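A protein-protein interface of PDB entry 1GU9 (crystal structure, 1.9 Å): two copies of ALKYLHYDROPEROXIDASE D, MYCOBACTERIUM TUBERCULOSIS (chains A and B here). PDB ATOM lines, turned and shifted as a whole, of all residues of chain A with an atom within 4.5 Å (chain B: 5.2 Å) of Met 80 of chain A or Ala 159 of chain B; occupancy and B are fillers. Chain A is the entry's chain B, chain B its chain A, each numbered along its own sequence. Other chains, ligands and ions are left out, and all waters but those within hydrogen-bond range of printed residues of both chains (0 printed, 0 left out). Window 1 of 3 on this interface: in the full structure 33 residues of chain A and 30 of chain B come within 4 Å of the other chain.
The side-chain amide oxygen of Asn 20 of chain B is in hydrogen-bond range of the backbone NH of Arg 103 of chain A (2.7 Å).
The side-chain sulfur (SD) of Met 80 of chain A sits at hydrogen-bond distance from the side-chain amide nitrogen (ND2) of Asn 20 of chain B, at 3.4 Å.
The backbone carbonyl oxygen of Ala 158 of chain B sits at hydrogen-bond distance from the side-chain hydroxyl of Ser 162 of chain B.
Among the printed residues, merely in contact across the chains: Met 80 of chain A with Ile 160 of chain B, Met 80 of chain A with Ala 159 of chain B, Leu 102 of chain A with Ile 160 of chain B, Gly 79 of chain A with Ser 162 of chain B, Leu 102 of chain A with Asn 20 of chain B, Val 83 of chain A with Ile 127 of chain B, Val 83 of chain A with Ser 162 of chain B, Val 83 of chain A with Ala 159 of chain B, Phe 84 of chain A with Ala 159 of chain B, Ala 76 of chain A with Gly 163 of chain B, Met 80 of chain A with Gly 163 of chain B, Phe 84 of chain A with Leu 155 of chain B and Phe 84 of chain A with Lys 156 of chain B.
Ala 159 of chain B touches three residues of chain A.
Printed residues of chain B within 4 Å of Arg 103 of chain A: Asn 20.
Of the printed residues of chain A, Gly 163 of chain B touches Ala 76 and Met 80.
Of the printed residues of chain A, Lys 156 of chain B touches Phe 84 (3.95 Å).
Printed residues of chain A within 4 Å of Leu 155 of chain B: Phe 84 (3.9 Å).
Printed residues of chain B within 4 Å of Ala 76 of chain A: Gly 163.
Ile 77 of chain A touches none of the printed residues of chain B.
The nearest residue of chain A that does not touch Ala 159 of chain B is Gly 79 of chain A (4.2 Å).
The nearest printed residue of chain A that does not touch Ser 162 of chain B is Met 80 of chain A (4.8 Å).
Printed residues of chain B that touch a printed residue of chain A: Asn 20, Ile 127, Leu 155, Lys 156, Ala 159, Ile 160, Ser 162 and Gly 163.
Hydrophobic or aromatic side chains of chain B within 4 Å of the printed part of chain A: Ile 127, Leu 155, Ala 159 and Ile 160.
Along chain B the printed residues that touch a printed residue of chain A span positions 20 to 163.
Of the 11 printed residues of chain A, 7 touch a printed residue of chain B.
Printed residues of chain A that touch a printed residue of chain B: Ala 76, Gly 79, Met 80, Val 83, Phe 84, Leu 102 and Arg 103.
Hydrophobic or aromatic side chains of chain A within 4 Å of the printed part of chain B: Met 80, Val 83, Phe 84 and Leu 102.
Among the printed residues, 15 pairs touch across the chains.
No position is printed for both chains.
Of the 15 pairs that touch across the chains among the printed residues, none has its exchanged pair printed and touching as well.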
ATOM      1  N   ALA A  76     -29.892  -6.458  -7.840  1.00  0.00           N
ATOM      2  CA  ALA A  76     -29.184  -7.716  -7.996  1.00  0.00           C
ATOM      3  C   ALA A  76     -27.713  -7.618  -7.686  1.00  0.00           C
ATOM      4  O   ALA A  76     -27.170  -8.443  -6.947  1.00  0.00           O
ATOM      5  CB  ALA A  76     -29.374  -8.257  -9.427  1.00  0.00           C
ATOM      6  N   ILE A  77     -27.046  -6.618  -8.250  1.00  0.00           N
ATOM      7  CA  ILE A  77     -25.626  -6.525  -8.023  1.00  0.00           C
ATOM      8  C   ILE A  77     -25.308  -6.075  -6.614  1.00  0.00           C
ATOM      9  O   ILE A  77     -24.312  -6.509  -6.040  1.00  0.00           O
ATOM     10  CB  ILE A  77     -24.920  -5.630  -9.058  1.00  0.00           C
ATOM     11  CG1 ILE A  77     -23.498  -6.164  -9.262  1.00  0.00           C
ATOM     12  CG2 ILE A  77     -24.911  -4.165  -8.615  1.00  0.00           C
ATOM     13  CD1 ILE A  77     -22.604  -5.228 -10.014  1.00  0.00           C
ATOM     14  N   MET A  78     -26.149  -5.223  -6.039  1.00  0.00           N
ATOM     15  CA  MET A  78     -25.883  -4.812  -4.658  1.00  0.00           C
ATOM     16  C   MET A  78     -26.107  -6.033  -3.751  1.00  0.00           C
ATOM     17  O   MET A  78     -25.492  -6.152  -2.683  1.00  0.00           O
ATOM     18  CB  MET A  78     -26.792  -3.660  -4.239  1.00  0.00           C
ATOM     19  CG  MET A  78     -26.322  -2.276  -4.760  1.00  0.00           C
ATOM     20  SD  MET A  78     -24.506  -1.875  -4.327  1.00  0.00           S
ATOM     21  CE  MET A  78     -24.803  -0.818  -2.740  1.00  0.00           C
ATOM     22  N   GLY A  79     -26.975  -6.937  -4.200  1.00  0.00           N
ATOM     23  CA  GLY A  79     -27.259  -8.148  -3.444  1.00  0.00           C
ATOM     24  C   GLY A  79     -25.976  -8.908  -3.117  1.00  0.00           C
ATOM     25  O   GLY A  79     -25.812  -9.473  -2.036  1.00  0.00           O
ATOM     26  N   MET A  80     -25.056  -8.939  -4.069  1.00  0.00           N
ATOM     27  CA  MET A  80     -23.780  -9.610  -3.855  1.00  0.00           C
ATOM     28  C   MET A  80     -22.764  -8.693  -3.156  1.00  0.00           C
ATOM     29  O   MET A  80     -22.123  -9.078  -2.171  1.00  0.00           O
ATOM     30  CB  MET A  80     -23.193 -10.057  -5.214  1.00  0.00           C
ATOM     31  CG  MET A  80     -21.689 -10.281  -5.166  1.00  0.00           C
ATOM     32  SD  MET A  80     -21.059 -10.800  -6.974  1.00  0.00           S
ATOM     33  CE  MET A  80     -20.638  -9.054  -7.670  1.00  0.00           C
ATOM     34  N   ASN A  81     -22.580  -7.494  -3.717  1.00  0.00           N
ATOM     35  CA  ASN A  81     -21.631  -6.526  -3.171  1.00  0.00           C
ATOM     36  C   ASN A  81     -21.897  -6.195  -1.708  1.00  0.00           C
ATOM     37  O   ASN A  81     -20.968  -6.103  -0.924  1.00  0.00           O
ATOM     38  CB  ASN A  81     -21.664  -5.227  -3.997  1.00  0.00           C
ATOM     39  CG  ASN A  81     -20.806  -5.315  -5.248  1.00  0.00           C
ATOM     40  OD1 ASN A  81     -20.365  -6.404  -5.630  1.00  0.00           O
ATOM     41  ND2 ASN A  81     -20.564  -4.174  -5.895  1.00  0.00           N
ATOM     42  N   ASN A  82     -23.159  -6.001  -1.354  1.00  0.00           N
ATOM     43  CA  ASN A  82     -23.502  -5.670   0.036  1.00  0.00           C
ATOM     44  C   ASN A  82     -23.084  -6.770   1.021  1.00  0.00           C
ATOM     45  O   ASN A  82     -22.919  -6.524   2.214  1.00  0.00           O
ATOM     46  CB  ASN A  82     -24.996  -5.391   0.166  1.00  0.00           C
ATOM     47  CG  ASN A  82     -25.391  -4.040  -0.399  1.00  0.00           C
ATOM     48  OD1 ASN A  82     -24.549  -3.160  -0.618  1.00  0.00           O
ATOM     49  ND2 ASN A  82     -26.662  -3.867  -0.625  1.00  0.00           N
ATOM     50  N   VAL A  83     -22.919  -7.990   0.530  1.00  0.00           N
ATOM     51  CA  VAL A  83     -22.480  -9.079   1.413  1.00  0.00           C
ATOM     52  C   VAL A  83     -20.965  -9.143   1.425  1.00  0.00           C
ATOM     53  O   VAL A  83     -20.336  -9.219   2.477  1.00  0.00           O
ATOM     54  CB  VAL A  83     -23.008 -10.425   0.938  1.00  0.00           C
ATOM     55  CG1 VAL A  83     -22.317 -11.558   1.705  1.00  0.00           C
ATOM     56  CG2 VAL A  83     -24.508 -10.474   1.104  1.00  0.00           C
ATOM     57  N   PHE A  84     -20.371  -9.066   0.238  1.00  0.00           N
ATOM     58  CA  PHE A  84     -18.937  -9.171   0.130  1.00  0.00           C
ATOM     59  C   PHE A  84     -18.185  -8.065   0.829  1.00  0.00           C
ATOM     60  O   PHE A  84     -17.313  -8.323   1.646  1.00  0.00           O
ATOM     61  CB  PHE A  84     -18.514  -9.186  -1.353  1.00  0.00           C
ATOM     62  CG  PHE A  84     -17.036  -9.214  -1.540  1.00  0.00           C
ATOM     63  CD1 PHE A  84     -16.339 -10.402  -1.410  1.00  0.00           C
ATOM     64  CD2 PHE A  84     -16.330  -8.044  -1.790  1.00  0.00           C
ATOM     65  CE1 PHE A  84     -14.970 -10.425  -1.519  1.00  0.00           C
ATOM     66  CE2 PHE A  84     -14.940  -8.064  -1.898  1.00  0.00           C
ATOM     67  CZ  PHE A  84     -14.268  -9.248  -1.763  1.00  0.00           C
ATOM     68  N   LEU A 102     -14.557 -10.564  -8.719  1.00  0.00           N
ATOM     69  CA  LEU A 102     -16.003 -10.538  -8.882  1.00  0.00           C
ATOM     70  C   LEU A 102     -16.385  -9.573  -9.999  1.00  0.00           C
ATOM     71  O   LEU A 102     -15.993  -8.418  -9.976  1.00  0.00           O
ATOM     72  CB  LEU A 102     -16.682 -10.092  -7.578  1.00  0.00           C
ATOM     73  CG  LEU A 102     -16.503 -10.949  -6.320  1.00  0.00           C
ATOM     74  CD1 LEU A 102     -17.362 -10.369  -5.188  1.00  0.00           C
ATOM     75  CD2 LEU A 102     -16.938 -12.382  -6.596  1.00  0.00           C
ATOM     76  N   ARG A 103     -17.150 -10.048 -10.979  1.00  0.00           N
ATOM     77  CA  ARG A 103     -17.556  -9.178 -12.083  1.00  0.00           C
ATOM     78  C   ARG A 103     -18.719  -8.303 -11.647  1.00  0.00           C
ATOM     79  O   ARG A 103     -19.664  -8.777 -11.017  1.00  0.00           O
ATOM     80  CB  ARG A 103     -17.965 -10.014 -13.292  1.00  0.00           C
ATOM     81  CG  ARG A 103     -16.855 -10.977 -13.754  1.00  0.00           C
ATOM     82  CD  ARG A 103     -15.680 -10.298 -14.456  1.00  0.00           C
ATOM     83  NE  ARG A 103     -15.837 -10.355 -15.908  1.00  0.00           N
ATOM     84  CZ  ARG A 103     -16.406  -9.409 -16.643  1.00  0.00           C
ATOM     85  NH1 ARG A 103     -16.872  -8.302 -16.072  1.00  0.00           N
ATOM     86  NH2 ARG A 103     -16.540  -9.587 -17.949  1.00  0.00           N
ATOM     87  N   ASN B  20     -20.578 -14.572 -12.450  1.00  0.00           N
ATOM     88  CA  ASN B  20     -19.939 -14.902 -11.179  1.00  0.00           C
ATOM     89  C   ASN B  20     -20.340 -16.287 -10.663  1.00  0.00           C
ATOM     90  O   ASN B  20     -19.532 -16.992 -10.044  1.00  0.00           O
ATOM     91  CB  ASN B  20     -20.271 -13.822 -10.126  1.00  0.00           C
ATOM     92  CG  ASN B  20     -19.537 -12.498 -10.364  1.00  0.00           C
ATOM     93  OD1 ASN B  20     -18.340 -12.484 -10.629  1.00  0.00           O
ATOM     94  ND2 ASN B  20     -20.253 -11.376 -10.217  1.00  0.00           N
ATOM     95  N   ILE B 127     -23.653 -13.647   5.186  1.00  0.00           N
ATOM     96  CA  ILE B 127     -24.961 -13.340   4.614  1.00  0.00           C
ATOM     97  C   ILE B 127     -25.842 -12.589   5.610  1.00  0.00           C
ATOM     98  O   ILE B 127     -26.478 -11.589   5.264  1.00  0.00           O
ATOM     99  CB  ILE B 127     -25.663 -14.624   4.130  1.00  0.00           C
ATOM    100  CG1 ILE B 127     -25.021 -15.095   2.810  1.00  0.00           C
ATOM    101  CG2 ILE B 127     -27.126 -14.356   3.770  1.00  0.00           C
ATOM    102  CD1 ILE B 127     -23.597 -14.742   2.684  1.00  0.00           C
ATOM    103  N   ALA B 154     -14.858 -18.596   0.295  1.00  0.00           N
ATOM    104  CA  ALA B 154     -16.167 -18.826   0.912  1.00  0.00           C
ATOM    105  C   ALA B 154     -16.945 -17.480   0.993  1.00  0.00           C
ATOM    106  O   ALA B 154     -18.152 -17.426   0.742  1.00  0.00           O
ATOM    107  CB  ALA B 154     -15.985 -19.418   2.305  1.00  0.00           C
ATOM    108  N   LEU B 155     -16.243 -16.412   1.358  1.00  0.00           N
ATOM    109  CA  LEU B 155     -16.877 -15.094   1.453  1.00  0.00           C
ATOM    110  C   LEU B 155     -17.414 -14.753   0.069  1.00  0.00           C
ATOM    111  O   LEU B 155     -18.553 -14.334  -0.072  1.00  0.00           O
ATOM    112  CB  LEU B 155     -15.872 -14.038   1.895  1.00  0.00           C
ATOM    113  CG  LEU B 155     -16.484 -12.624   1.941  1.00  0.00           C
ATOM    114  CD1 LEU B 155     -17.691 -12.586   2.912  1.00  0.00           C
ATOM    115  CD2 LEU B 155     -15.454 -11.658   2.366  1.00  0.00           C
ATOM    116  N   LYS B 156     -16.593 -14.955  -0.968  1.00  0.00           N
ATOM    117  CA  LYS B 156     -17.041 -14.684  -2.341  1.00  0.00           C
ATOM    118  C   LYS B 156     -18.303 -15.497  -2.709  1.00  0.00           C
ATOM    119  O   LYS B 156     -19.276 -14.965  -3.261  1.00  0.00           O
ATOM    120  CB  LYS B 156     -15.891 -14.996  -3.329  1.00  0.00           C
ATOM    121  CG  LYS B 156     -14.774 -13.926  -3.346  1.00  0.00           C
ATOM    122  CD  LYS B 156     -13.470 -14.439  -4.002  1.00  0.00           C
ATOM    123  CE  LYS B 156     -13.665 -14.836  -5.461  1.00  0.00           C
ATOM    124  NZ  LYS B 156     -12.411 -15.433  -6.037  1.00  0.00           N
ATOM    125  N   ALA B 157     -18.290 -16.790  -2.396  1.00  0.00           N
ATOM    126  CA  ALA B 157     -19.419 -17.666  -2.709  1.00  0.00           C
ATOM    127  C   ALA B 157     -20.708 -17.230  -2.008  1.00  0.00           C
ATOM    128  O   ALA B 157     -21.780 -17.216  -2.611  1.00  0.00           O
ATOM    129  CB  ALA B 157     -19.091 -19.099  -2.304  1.00  0.00           C
ATOM    130  N   ALA B 158     -20.597 -16.931  -0.717  1.00  0.00           N
ATOM    131  CA  ALA B 158     -21.772 -16.490   0.032  1.00  0.00           C
ATOM    132  C   ALA B 158     -22.360 -15.242  -0.635  1.00  0.00           C
ATOM    133  O   ALA B 158     -23.564 -15.139  -0.801  1.00  0.00           O
ATOM    134  CB  ALA B 158     -21.378 -16.208   1.461  1.00  0.00           C
ATOM    135  N   ALA B 159     -21.499 -14.292  -1.003  1.00  0.00           N
ATOM    136  CA  ALA B 159     -21.960 -13.061  -1.652  1.00  0.00           C
ATOM    137  C   ALA B 159     -22.599 -13.371  -3.020  1.00  0.00           C
ATOM    138  O   ALA B 159     -23.696 -12.906  -3.330  1.00  0.00           O
ATOM    139  CB  ALA B 159     -20.800 -12.106  -1.844  1.00  0.00           C
ATOM    140  N   ILE B 160     -21.916 -14.175  -3.827  1.00  0.00           N
ATOM    141  CA  ILE B 160     -22.437 -14.520  -5.152  1.00  0.00           C
ATOM    142  C   ILE B 160     -23.810 -15.148  -5.027  1.00  0.00           C
ATOM    143  O   ILE B 160     -24.735 -14.782  -5.745  1.00  0.00           O
ATOM    144  CB  ILE B 160     -21.530 -15.541  -5.893  1.00  0.00           C
ATOM    145  CG1 ILE B 160     -20.119 -14.990  -6.064  1.00  0.00           C
ATOM    146  CG2 ILE B 160     -22.136 -15.877  -7.240  1.00  0.00           C
ATOM    147  CD1 ILE B 160     -20.048 -13.733  -6.861  1.00  0.00           C
ATOM    148  N   VAL B 161     -23.942 -16.109  -4.118  1.00  0.00           N
ATOM    149  CA  VAL B 161     -25.228 -16.770  -3.928  1.00  0.00           C
ATOM    150  C   VAL B 161     -26.317 -15.802  -3.459  1.00  0.00           C
ATOM    151  O   VAL B 161     -27.487 -15.953  -3.823  1.00  0.00           O
ATOM    152  CB  VAL B 161     -25.098 -17.971  -2.953  1.00  0.00           C
ATOM    153  CG1 VAL B 161     -26.456 -18.517  -2.624  1.00  0.00           C
ATOM    154  CG2 VAL B 161     -24.298 -19.087  -3.629  1.00  0.00           C
ATOM    155  N   SER B 162     -25.948 -14.794  -2.672  1.00  0.00           N
ATOM    156  CA  SER B 162     -26.947 -13.817  -2.246  1.00  0.00           C
ATOM    157  C   SER B 162     -27.421 -13.060  -3.498  1.00  0.00           C
ATOM    158  O   SER B 162     -28.614 -12.807  -3.692  1.00  0.00           O
ATOM    159  CB  SER B 162     -26.322 -12.839  -1.254  1.00  0.00           C
ATOM    160  OG  SER B 162     -25.938 -13.530  -0.085  1.00  0.00           O
ATOM    161  N   GLY B 163     -26.476 -12.708  -4.357  1.00  0.00           N
ATOM    162  CA  GLY B 163     -26.848 -12.009  -5.574  1.00  0.00           C
ATOM    163  C   GLY B 163     -27.787 -12.879  -6.400  1.00  0.00           C
ATOM    164  O   GLY B 163     -28.799 -12.418  -6.925  1.00  0.00           O
ATOM    165  N   VAL B 164     -27.440 -14.155  -6.518  1.00  0.00           N
ATOM    166  CA  VAL B 164     -28.261 -15.058  -7.297  1.00  0.00           C
ATOM    167  C   VAL B 164     -29.684 -15.094  -6.767  1.00  0.00           C
ATOM    168  O   VAL B 164     -30.625 -15.032  -7.537  1.00  0.00           O
ATOM    169  CB  VAL B 164     -27.709 -16.516  -7.292  1.00  0.00           C
ATOM    170  CG1 VAL B 164     -28.681 -17.427  -8.012  1.00  0.00           C
ATOM    171  CG2 VAL B 164     -26.330 -16.572  -7.966  1.00  0.00           C
